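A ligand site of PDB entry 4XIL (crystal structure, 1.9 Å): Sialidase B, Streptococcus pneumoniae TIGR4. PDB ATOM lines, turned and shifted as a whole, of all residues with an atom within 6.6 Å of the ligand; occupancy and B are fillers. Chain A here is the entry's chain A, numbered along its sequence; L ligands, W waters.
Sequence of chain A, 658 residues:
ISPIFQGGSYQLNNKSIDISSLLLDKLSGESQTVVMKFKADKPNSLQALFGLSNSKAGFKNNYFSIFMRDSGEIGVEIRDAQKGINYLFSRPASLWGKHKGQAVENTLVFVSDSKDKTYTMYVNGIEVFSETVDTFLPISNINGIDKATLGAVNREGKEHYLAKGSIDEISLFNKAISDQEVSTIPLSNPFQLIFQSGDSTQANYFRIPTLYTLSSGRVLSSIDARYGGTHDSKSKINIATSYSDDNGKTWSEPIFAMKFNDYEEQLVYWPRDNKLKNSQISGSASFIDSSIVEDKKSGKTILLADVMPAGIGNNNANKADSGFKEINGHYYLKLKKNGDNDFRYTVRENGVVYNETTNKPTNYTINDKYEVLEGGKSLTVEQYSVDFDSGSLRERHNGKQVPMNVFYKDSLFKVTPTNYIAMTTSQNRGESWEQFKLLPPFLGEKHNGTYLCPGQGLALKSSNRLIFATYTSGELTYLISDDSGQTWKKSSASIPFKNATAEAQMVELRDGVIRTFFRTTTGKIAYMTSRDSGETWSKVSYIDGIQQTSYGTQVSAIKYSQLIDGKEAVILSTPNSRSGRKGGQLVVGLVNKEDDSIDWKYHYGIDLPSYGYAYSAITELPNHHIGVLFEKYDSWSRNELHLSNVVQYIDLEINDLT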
ATOM      1  N   LEU A 211      -4.319 -33.585 -21.894  1.00  0.00           N
ATOM      2  CA  LEU A 211      -2.981 -33.482 -21.339  1.00  0.00           C
ATOM      3  C   LEU A 211      -2.653 -32.016 -21.166  1.00  0.00           C
ATOM      4  O   LEU A 211      -3.041 -31.190 -21.999  1.00  0.00           O
ATOM      5  CB  LEU A 211      -1.930 -34.108 -22.266  1.00  0.00           C
ATOM      6  CG  LEU A 211      -1.859 -35.644 -22.360  1.00  0.00           C
ATOM      7  CD1 LEU A 211      -0.910 -36.063 -23.487  1.00  0.00           C
ATOM      8  CD2 LEU A 211      -1.407 -36.262 -21.034  1.00  0.00           C
ATOM      9  N   TYR A 212      -1.902 -31.692 -20.115  1.00  0.00           N
ATOM     10  CA  TYR A 212      -1.522 -30.320 -19.855  1.00  0.00           C
ATOM     11  C   TYR A 212      -0.256 -30.302 -18.987  1.00  0.00           C
ATOM     12  O   TYR A 212      -0.158 -31.026 -17.983  1.00  0.00           O
ATOM     13  CB  TYR A 212      -2.665 -29.571 -19.160  1.00  0.00           C
ATOM     14  CG  TYR A 212      -2.494 -28.061 -19.129  1.00  0.00           C
ATOM     15  CD1 TYR A 212      -1.595 -27.462 -18.253  1.00  0.00           C
ATOM     16  CD2 TYR A 212      -3.260 -27.236 -19.969  1.00  0.00           C
ATOM     17  CE1 TYR A 212      -1.437 -26.066 -18.221  1.00  0.00           C
ATOM     18  CE2 TYR A 212      -3.102 -25.840 -19.937  1.00  0.00           C
ATOM     19  CZ  TYR A 212      -2.192 -25.271 -19.065  1.00  0.00           C
ATOM     20  OH  TYR A 212      -2.025 -23.893 -19.025  1.00  0.00           O
ATOM     21  N   THR A 213       0.727 -29.505 -19.386  1.00  0.00           N
ATOM     22  CA  THR A 213       2.004 -29.473 -18.669  1.00  0.00           C
ATOM     23  C   THR A 213       2.018 -28.318 -17.662  1.00  0.00           C
ATOM     24  O   THR A 213       1.884 -27.162 -18.047  1.00  0.00           O
ATOM     25  CB  THR A 213       3.192 -29.356 -19.657  1.00  0.00           C
ATOM     26  OG1 THR A 213       3.106 -30.387 -20.647  1.00  0.00           O
ATOM     27  CG2 THR A 213       4.535 -29.483 -18.895  1.00  0.00           C
ATOM     28  N   LEU A 214       2.188 -28.655 -16.388  1.00  0.00           N
ATOM     29  CA  LEU A 214       2.133 -27.665 -15.323  1.00  0.00           C
ATOM     30  C   LEU A 214       3.509 -27.044 -15.067  1.00  0.00           C
ATOM     31  O   LEU A 214       4.547 -27.607 -15.438  1.00  0.00           O
ATOM     32  CB  LEU A 214       1.590 -28.280 -14.036  1.00  0.00           C
ATOM     33  CG  LEU A 214       0.263 -29.026 -14.193  1.00  0.00           C
ATOM     34  CD1 LEU A 214      -0.084 -29.776 -12.906  1.00  0.00           C
ATOM     35  CD2 LEU A 214      -0.850 -28.034 -14.591  1.00  0.00           C
ATOM     36  N   GLU A 294      -3.862 -24.033 -16.263  1.00  0.00           N
ATOM     37  CA  GLU A 294      -3.187 -23.646 -15.025  1.00  0.00           C
ATOM     38  C   GLU A 294      -3.083 -22.139 -14.934  1.00  0.00           C
ATOM     39  O   GLU A 294      -2.728 -21.482 -15.904  1.00  0.00           O
ATOM     40  CB  GLU A 294      -1.800 -24.279 -14.917  1.00  0.00           C
ATOM     41  CG  GLU A 294      -1.185 -24.085 -13.518  1.00  0.00           C
ATOM     42  CD  GLU A 294       0.202 -24.703 -13.368  1.00  0.00           C
ATOM     43  OE1 GLU A 294       1.023 -24.537 -14.297  1.00  0.00           O
ATOM     44  OE2 GLU A 294       0.457 -25.350 -12.330  1.00  0.00           O
ATOM     45  N   GLN A 456      -7.355 -28.589 -23.622  1.00  0.00           N
ATOM     46  CA  GLN A 456      -6.706 -27.574 -22.808  1.00  0.00           C
ATOM     47  C   GLN A 456      -7.457 -26.263 -22.888  1.00  0.00           C
ATOM     48  O   GLN A 456      -7.994 -25.919 -23.943  1.00  0.00           O
ATOM     49  CB  GLN A 456      -5.285 -27.337 -23.299  1.00  0.00           C
ATOM     50  CG  GLN A 456      -4.413 -28.579 -23.460  1.00  0.00           C
ATOM     51  CD  GLN A 456      -2.989 -28.206 -23.825  1.00  0.00           C
ATOM     52  OE1 GLN A 456      -2.722 -27.085 -24.278  1.00  0.00           O
ATOM     53  NE2 GLN A 456      -2.066 -29.135 -23.627  1.00  0.00           N
ATOM     54  N   GLY A 457      -7.470 -25.527 -21.787  1.00  0.00           N
ATOM     55  CA  GLY A 457      -7.785 -24.105 -21.861  1.00  0.00           C
ATOM     56  C   GLY A 457      -6.499 -23.372 -22.200  1.00  0.00           C
ATOM     57  O   GLY A 457      -5.447 -24.010 -22.356  1.00  0.00           O
ATOM     58  N   LEU A 458      -6.546 -22.049 -22.302  1.00  0.00           N
ATOM     59  CA  LEU A 458      -5.362 -21.300 -22.653  1.00  0.00           C
ATOM     60  C   LEU A 458      -5.079 -20.226 -21.604  1.00  0.00           C
ATOM     61  O   LEU A 458      -5.945 -19.413 -21.291  1.00  0.00           O
ATOM     62  CB  LEU A 458      -5.528 -20.648 -24.015  1.00  0.00           C
ATOM     63  CG  LEU A 458      -4.379 -19.708 -24.424  1.00  0.00           C
ATOM     64  CD1 LEU A 458      -3.057 -20.466 -24.619  1.00  0.00           C
ATOM     65  CD2 LEU A 458      -4.763 -18.921 -25.688  1.00  0.00           C
ATOM     66  N   ALA A 459      -3.873 -20.263 -21.047  1.00  0.00           N
ATOM     67  CA  ALA A 459      -3.390 -19.202 -20.169  1.00  0.00           C
ATOM     68  C   ALA A 459      -2.497 -18.271 -20.972  1.00  0.00           C
ATOM     69  O   ALA A 459      -1.436 -18.668 -21.429  1.00  0.00           O
ATOM     70  CB  ALA A 459      -2.612 -19.802 -18.978  1.00  0.00           C
ATOM     71  N   LYS A 461       0.250 -15.629 -21.970  1.00  0.00           N
ATOM     72  CA  LYS A 461       1.584 -15.546 -21.405  1.00  0.00           C
ATOM     73  C   LYS A 461       1.847 -14.228 -20.684  1.00  0.00           C
ATOM     74  O   LYS A 461       2.515 -14.212 -19.657  1.00  0.00           O
ATOM     75  CB  LYS A 461       2.641 -15.733 -22.500  1.00  0.00           C
ATOM     76  CG  LYS A 461       2.655 -17.117 -23.145  1.00  0.00           C
ATOM     77  CD  LYS A 461       2.860 -18.219 -22.114  1.00  0.00           C
ATOM     78  CE  LYS A 461       3.395 -19.491 -22.758  1.00  0.00           C
ATOM     79  NZ  LYS A 461       2.450 -20.110 -23.758  1.00  0.00           N
ATOM     80  N   ALA A 557      -4.010 -29.079 -30.330  1.00  0.00           N
ATOM     81  CA  ALA A 557      -3.047 -28.152 -30.907  1.00  0.00           C
ATOM     82  C   ALA A 557      -2.207 -27.506 -29.814  1.00  0.00           C
ATOM     83  O   ALA A 557      -2.731 -27.102 -28.788  1.00  0.00           O
ATOM     84  CB  ALA A 557      -3.759 -27.060 -31.696  1.00  0.00           C
ATOM     85  N   ILE A 558      -0.896 -27.418 -30.054  1.00  0.00           N
ATOM     86  CA  ILE A 558      -0.001 -26.713 -29.141  1.00  0.00           C
ATOM     87  C   ILE A 558       0.996 -25.855 -29.904  1.00  0.00           C
ATOM     88  O   ILE A 558       1.276 -26.086 -31.085  1.00  0.00           O
ATOM     89  CB  ILE A 558       0.814 -27.679 -28.257  1.00  0.00           C
ATOM     90  CG1 ILE A 558       1.696 -28.575 -29.124  1.00  0.00           C
ATOM     91  CG2 ILE A 558      -0.114 -28.447 -27.322  1.00  0.00           C
ATOM     92  CD1 ILE A 558       2.639 -29.474 -28.339  1.00  0.00           C
ATOM     93  N   LYS A 559       1.512 -24.852 -29.212  1.00  0.00           N
ATOM     94  CA  LYS A 559       2.635 -24.076 -29.699  1.00  0.00           C
ATOM     95  C   LYS A 559       3.913 -24.645 -29.081  1.00  0.00           C
ATOM     96  O   LYS A 559       4.059 -24.656 -27.867  1.00  0.00           O
ATOM     97  CB  LYS A 559       2.456 -22.620 -29.284  1.00  0.00           C
ATOM     98  CG  LYS A 559       3.638 -21.723 -29.582  1.00  0.00           C
ATOM     99  CD  LYS A 559       3.731 -21.466 -31.064  1.00  0.00           C
ATOM    100  CE  LYS A 559       4.802 -20.432 -31.367  1.00  0.00           C
ATOM    101  NZ  LYS A 559       6.160 -21.018 -31.163  1.00  0.00           N
ATOM    102  N   SER A 561       7.752 -24.986 -27.821  1.00  0.00           N
ATOM    103  CA  SER A 561       8.558 -23.966 -27.150  1.00  0.00           C
ATOM    104  C   SER A 561       9.847 -23.657 -27.908  1.00  0.00           C
ATOM    105  O   SER A 561      10.433 -22.582 -27.733  1.00  0.00           O
ATOM    106  CB  SER A 561       8.904 -24.383 -25.715  1.00  0.00           C
ATOM    107  OG  SER A 561       9.878 -25.409 -25.714  1.00  0.00           O
ATOM    108  N   GLN A 562      10.312 -24.611 -28.708  1.00  0.00           N
ATOM    109  CA  GLN A 562      11.582 -24.461 -29.417  1.00  0.00           C
ATOM    110  C   GLN A 562      11.379 -24.183 -30.897  1.00  0.00           C
ATOM    111  O   GLN A 562      10.389 -24.619 -31.490  1.00  0.00           O
ATOM    112  CB  GLN A 562      12.444 -25.707 -29.250  1.00  0.00           C
ATOM    113  CG  GLN A 562      12.570 -26.193 -27.813  1.00  0.00           C
ATOM    114  CD  GLN A 562      13.343 -25.226 -26.941  1.00  0.00           C
ATOM    115  OE1 GLN A 562      14.488 -24.874 -27.250  1.00  0.00           O
ATOM    116  NE2 GLN A 562      12.725 -24.787 -25.851  1.00  0.00           N
ATOM    117  N   ILE A 618      -2.428 -33.556 -26.812  1.00  0.00           N
ATOM    118  CA  ILE A 618      -0.998 -33.436 -27.010  1.00  0.00           C
ATOM    119  C   ILE A 618      -0.461 -32.381 -26.069  1.00  0.00           C
ATOM    120  O   ILE A 618      -1.137 -31.395 -25.798  1.00  0.00           O
ATOM    121  CB  ILE A 618      -0.674 -33.073 -28.457  1.00  0.00           C
ATOM    122  CG1 ILE A 618      -0.836 -34.295 -29.343  1.00  0.00           C
ATOM    123  CG2 ILE A 618       0.776 -32.579 -28.595  1.00  0.00           C
ATOM    124  CD1 ILE A 618       0.120 -34.265 -30.460  1.00  0.00           C
ATOM    125  N   THR A 619       0.733 -32.615 -25.538  1.00  0.00           N
ATOM    126  CA  THR A 619       1.378 -31.574 -24.756  1.00  0.00           C
ATOM    127  C   THR A 619       2.902 -31.709 -24.884  1.00  0.00           C
ATOM    128  O   THR A 619       3.442 -32.811 -25.035  1.00  0.00           O
ATOM    129  CB  THR A 619       0.934 -31.603 -23.266  1.00  0.00           C
ATOM    130  OG1 THR A 619       1.241 -30.343 -22.654  1.00  0.00           O
ATOM    131  CG2 THR A 619       1.649 -32.717 -22.489  1.00  0.00           C
ATOM    132  N   GLU A 620       3.585 -30.566 -24.850  1.00  0.00           N
ATOM    133  CA  GLU A 620       5.032 -30.627 -24.778  1.00  0.00           C
ATOM    134  C   GLU A 620       5.434 -30.973 -23.333  1.00  0.00           C
ATOM    135  O   GLU A 620       5.095 -30.268 -22.379  1.00  0.00           O
ATOM    136  CB  GLU A 620       5.657 -29.293 -25.214  1.00  0.00           C
ATOM    137  CG  GLU A 620       7.183 -29.331 -25.219  1.00  0.00           C
ATOM    138  CD  GLU A 620       7.780 -28.002 -25.667  1.00  0.00           C
ATOM    139  OE1 GLU A 620       7.006 -27.110 -26.094  1.00  0.00           O
ATOM    140  OE2 GLU A 620       9.020 -27.848 -25.606  1.00  0.00           O
ATOM    141  N   LEU A 621       6.130 -32.101 -23.181  1.00  0.00           N
ATOM    142  CA  LEU A 621       6.660 -32.508 -21.876  1.00  0.00           C
ATOM    143  C   LEU A 621       7.793 -31.548 -21.488  1.00  0.00           C
ATOM    144  O   LEU A 621       8.351 -30.872 -22.354  1.00  0.00           O
ATOM    145  CB  LEU A 621       7.155 -33.943 -21.949  1.00  0.00           C
ATOM    146  CG  LEU A 621       6.063 -34.893 -22.476  1.00  0.00           C
ATOM    147  CD1 LEU A 621       6.586 -36.272 -22.806  1.00  0.00           C
ATOM    148  CD2 LEU A 621       4.936 -34.967 -21.460  1.00  0.00           C
ATOM    149  N   PRO A 622       8.102 -31.457 -20.192  1.00  0.00           N
ATOM    150  CA  PRO A 622       9.154 -30.513 -19.756  1.00  0.00           C
ATOM    151  C   PRO A 622      10.506 -30.752 -20.407  1.00  0.00           C
ATOM    152  O   PRO A 622      11.260 -29.780 -20.526  1.00  0.00           O
ATOM    153  CB  PRO A 622       9.241 -30.773 -18.245  1.00  0.00           C
ATOM    154  CG  PRO A 622       7.832 -31.154 -17.880  1.00  0.00           C
ATOM    155  CD  PRO A 622       7.308 -31.960 -19.052  1.00  0.00           C
ATOM    156  N   ASN A 623      10.812 -31.978 -20.826  1.00  0.00           N
ATOM    157  CA  ASN A 623      12.068 -32.264 -21.511  1.00  0.00           C
ATOM    158  C   ASN A 623      12.026 -32.028 -23.021  1.00  0.00           C
ATOM    159  O   ASN A 623      12.915 -32.469 -23.743  1.00  0.00           O
ATOM    160  CB  ASN A 623      12.525 -33.704 -21.240  1.00  0.00           C
ATOM    161  CG  ASN A 623      11.515 -34.734 -21.760  1.00  0.00           C
ATOM    162  OD1 ASN A 623      10.501 -34.369 -22.342  1.00  0.00           O
ATOM    163  ND2 ASN A 623      11.799 -36.022 -21.550  1.00  0.00           N
ATOM    164  N   HIS A 624      10.966 -31.361 -23.481  1.00  0.00           N
ATOM    165  CA  HIS A 624      10.748 -31.048 -24.907  1.00  0.00           C
ATOM    166  C   HIS A 624      10.381 -32.236 -25.789  1.00  0.00           C
ATOM    167  O   HIS A 624      10.334 -32.110 -27.008  1.00  0.00           O
ATOM    168  CB  HIS A 624      11.926 -30.246 -25.493  1.00  0.00           C
ATOM    169  CG  HIS A 624      12.314 -29.070 -24.645  1.00  0.00           C
ATOM    170  ND1 HIS A 624      11.417 -28.068 -24.333  1.00  0.00           N
ATOM    171  CD2 HIS A 624      13.465 -28.760 -24.015  1.00  0.00           C
ATOM    172  CE1 HIS A 624      12.008 -27.177 -23.559  1.00  0.00           C
ATOM    173  NE2 HIS A 624      13.256 -27.573 -23.345  1.00  0.00           N
HETATM  174  C1  LIG L   1       8.084 -26.908 -21.841  1.00  0.00           C
HETATM  175  C2  LIG L   1       8.086 -25.508 -21.249  1.00  0.00           C
HETATM  176  C3  LIG L   1       6.819 -27.628 -21.590  1.00  0.00           C
HETATM  177  C4  LIG L   1       6.849 -24.734 -21.544  1.00  0.00           C
HETATM  178  C5  LIG L   1       5.629 -26.807 -21.964  1.00  0.00           C
HETATM  179  C6  LIG L   1       3.182 -25.200 -21.030  1.00  0.00           C
HETATM  180  C7  LIG L   1       1.675 -25.284 -23.064  1.00  0.00           C
HETATM  181  C8  LIG L   1       0.687 -25.448 -20.881  1.00  0.00           C
HETATM  182  C9  LIG L   1       0.296 -25.815 -23.145  1.00  0.00           C
HETATM  183  C10 LIG L   1       0.117 -26.468 -21.826  1.00  0.00           C
HETATM  184  C11 LIG L   1       5.609 -25.505 -21.231  1.00  0.00           C
HETATM  185  C12 LIG L   1       1.851 -24.831 -21.643  1.00  0.00           C
HETATM  186  N1  LIG L   1       4.425 -24.685 -21.626  1.00  0.00           N
HETATM  187  O1  LIG L   1       1.704 -22.557 -20.167  1.00  0.00           O
HETATM  188  O2  LIG L   1       0.481 -22.648 -22.240  1.00  0.00           O
HETATM  189  O3  LIG L   1       0.186 -26.732 -24.185  1.00  0.00           O
HETATM  190  O4  LIG L   1       0.847 -27.607 -21.723  1.00  0.00           O
HETATM  191  O5  LIG L   1       2.903 -22.472 -22.320  1.00  0.00           O
HETATM  192  S1  LIG L   1       1.730 -23.036 -21.607  1.00  0.00           S
HETATM  193  O   HOH W   1       4.644 -22.322 -19.897  1.00  0.00           O
HETATM  194  O   HOH W   2       0.171 -22.935 -18.144  1.00  0.00           O
HETATM  195  O   HOH W   3       2.573 -28.038 -24.996  1.00  0.00           O
HETATM  196  O   HOH W   4       0.460 -24.600 -26.436  1.00  0.00           O
HETATM  197  O   HOH W   5       2.736 -22.684 -25.609  1.00  0.00           O
HETATM  198  O   HOH W   6      -2.109 -22.564 -21.486  1.00  0.00           O
HETATM  199  O   HOH W   7       4.739 -24.086 -24.270  1.00  0.00           O
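OG1 of Thr 619 lies within hydrogen-bond range of OG1 of Thr 213 (2.7 Å). The backbone carbonyl oxygen of Ile 618 sits at hydrogen-bond distance from the side-chain amide nitrogen of Gln 456, 3.3 Å away. O of Leu 211 sits at hydrogen-bond distance from NE2 of Gln 456, at 2.8 Å. OG1 of Thr 213 is in hydrogen-bond range of O of Glu 620 (2.6 Å). A ring nitrogen (ND1) of His 624 sits at hydrogen-bond distance from the side-chain carboxylate (OE2) of Glu 620 (2.7 Å). The side-chain carboxylate (OE2) of Glu 620 sits at hydrogen-bond distance from the side-chain hydroxyl (OG) of Ser 561 (2.6 Å). The backbone NH (N) of Glu 294 sits at hydrogen-bond distance from the side-chain hydroxyl (OH) of Tyr 212 (3.3 Å).
An oxygen (O5) of the ligand is in salt-bridge range of the side-chain amino group (NZ) of Lys 461, 2.8 Å away. The side-chain hydroxyl (OG1) of Thr 619 is in hydrogen-bond range of an oxygen (O4) of the ligand (2.9 Å). OE1 of Gln 456 lies within hydrogen-bond range of O3 of the ligand (2.9 Å). O4 of the ligand lies within hydrogen-bond range of N of Thr 213, 3.0 Å away.
Water W2 bridges OH of Tyr 212 (2.6 Å) and O1 of the ligand (2.6 Å). Water W6 lies within hydrogen-bond range of O2 of the ligand, OH of Tyr 212 and N of Ala 459. Water W3 lies within hydrogen-bond range of the backbone NH (N) of Glu 620 and an oxygen (O3) of the ligand. Water W4 bridges the backbone NH of Lys 559 (3.0 Å) and an oxygen (O3) of the ligand (3.1 Å). Water W5 lies within hydrogen-bond range of NZ of Lys 461, O of Lys 559 and O5 of the ligand.
Merely in contact with the ligand: Tyr 212, Ile 558, Glu 620 and Leu 621. Hydrophobic or aromatic side chains that line the ligand: Tyr 212 and Ile 558. Of the 22 residues printed, 8 come within 4 Å of the ligand.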
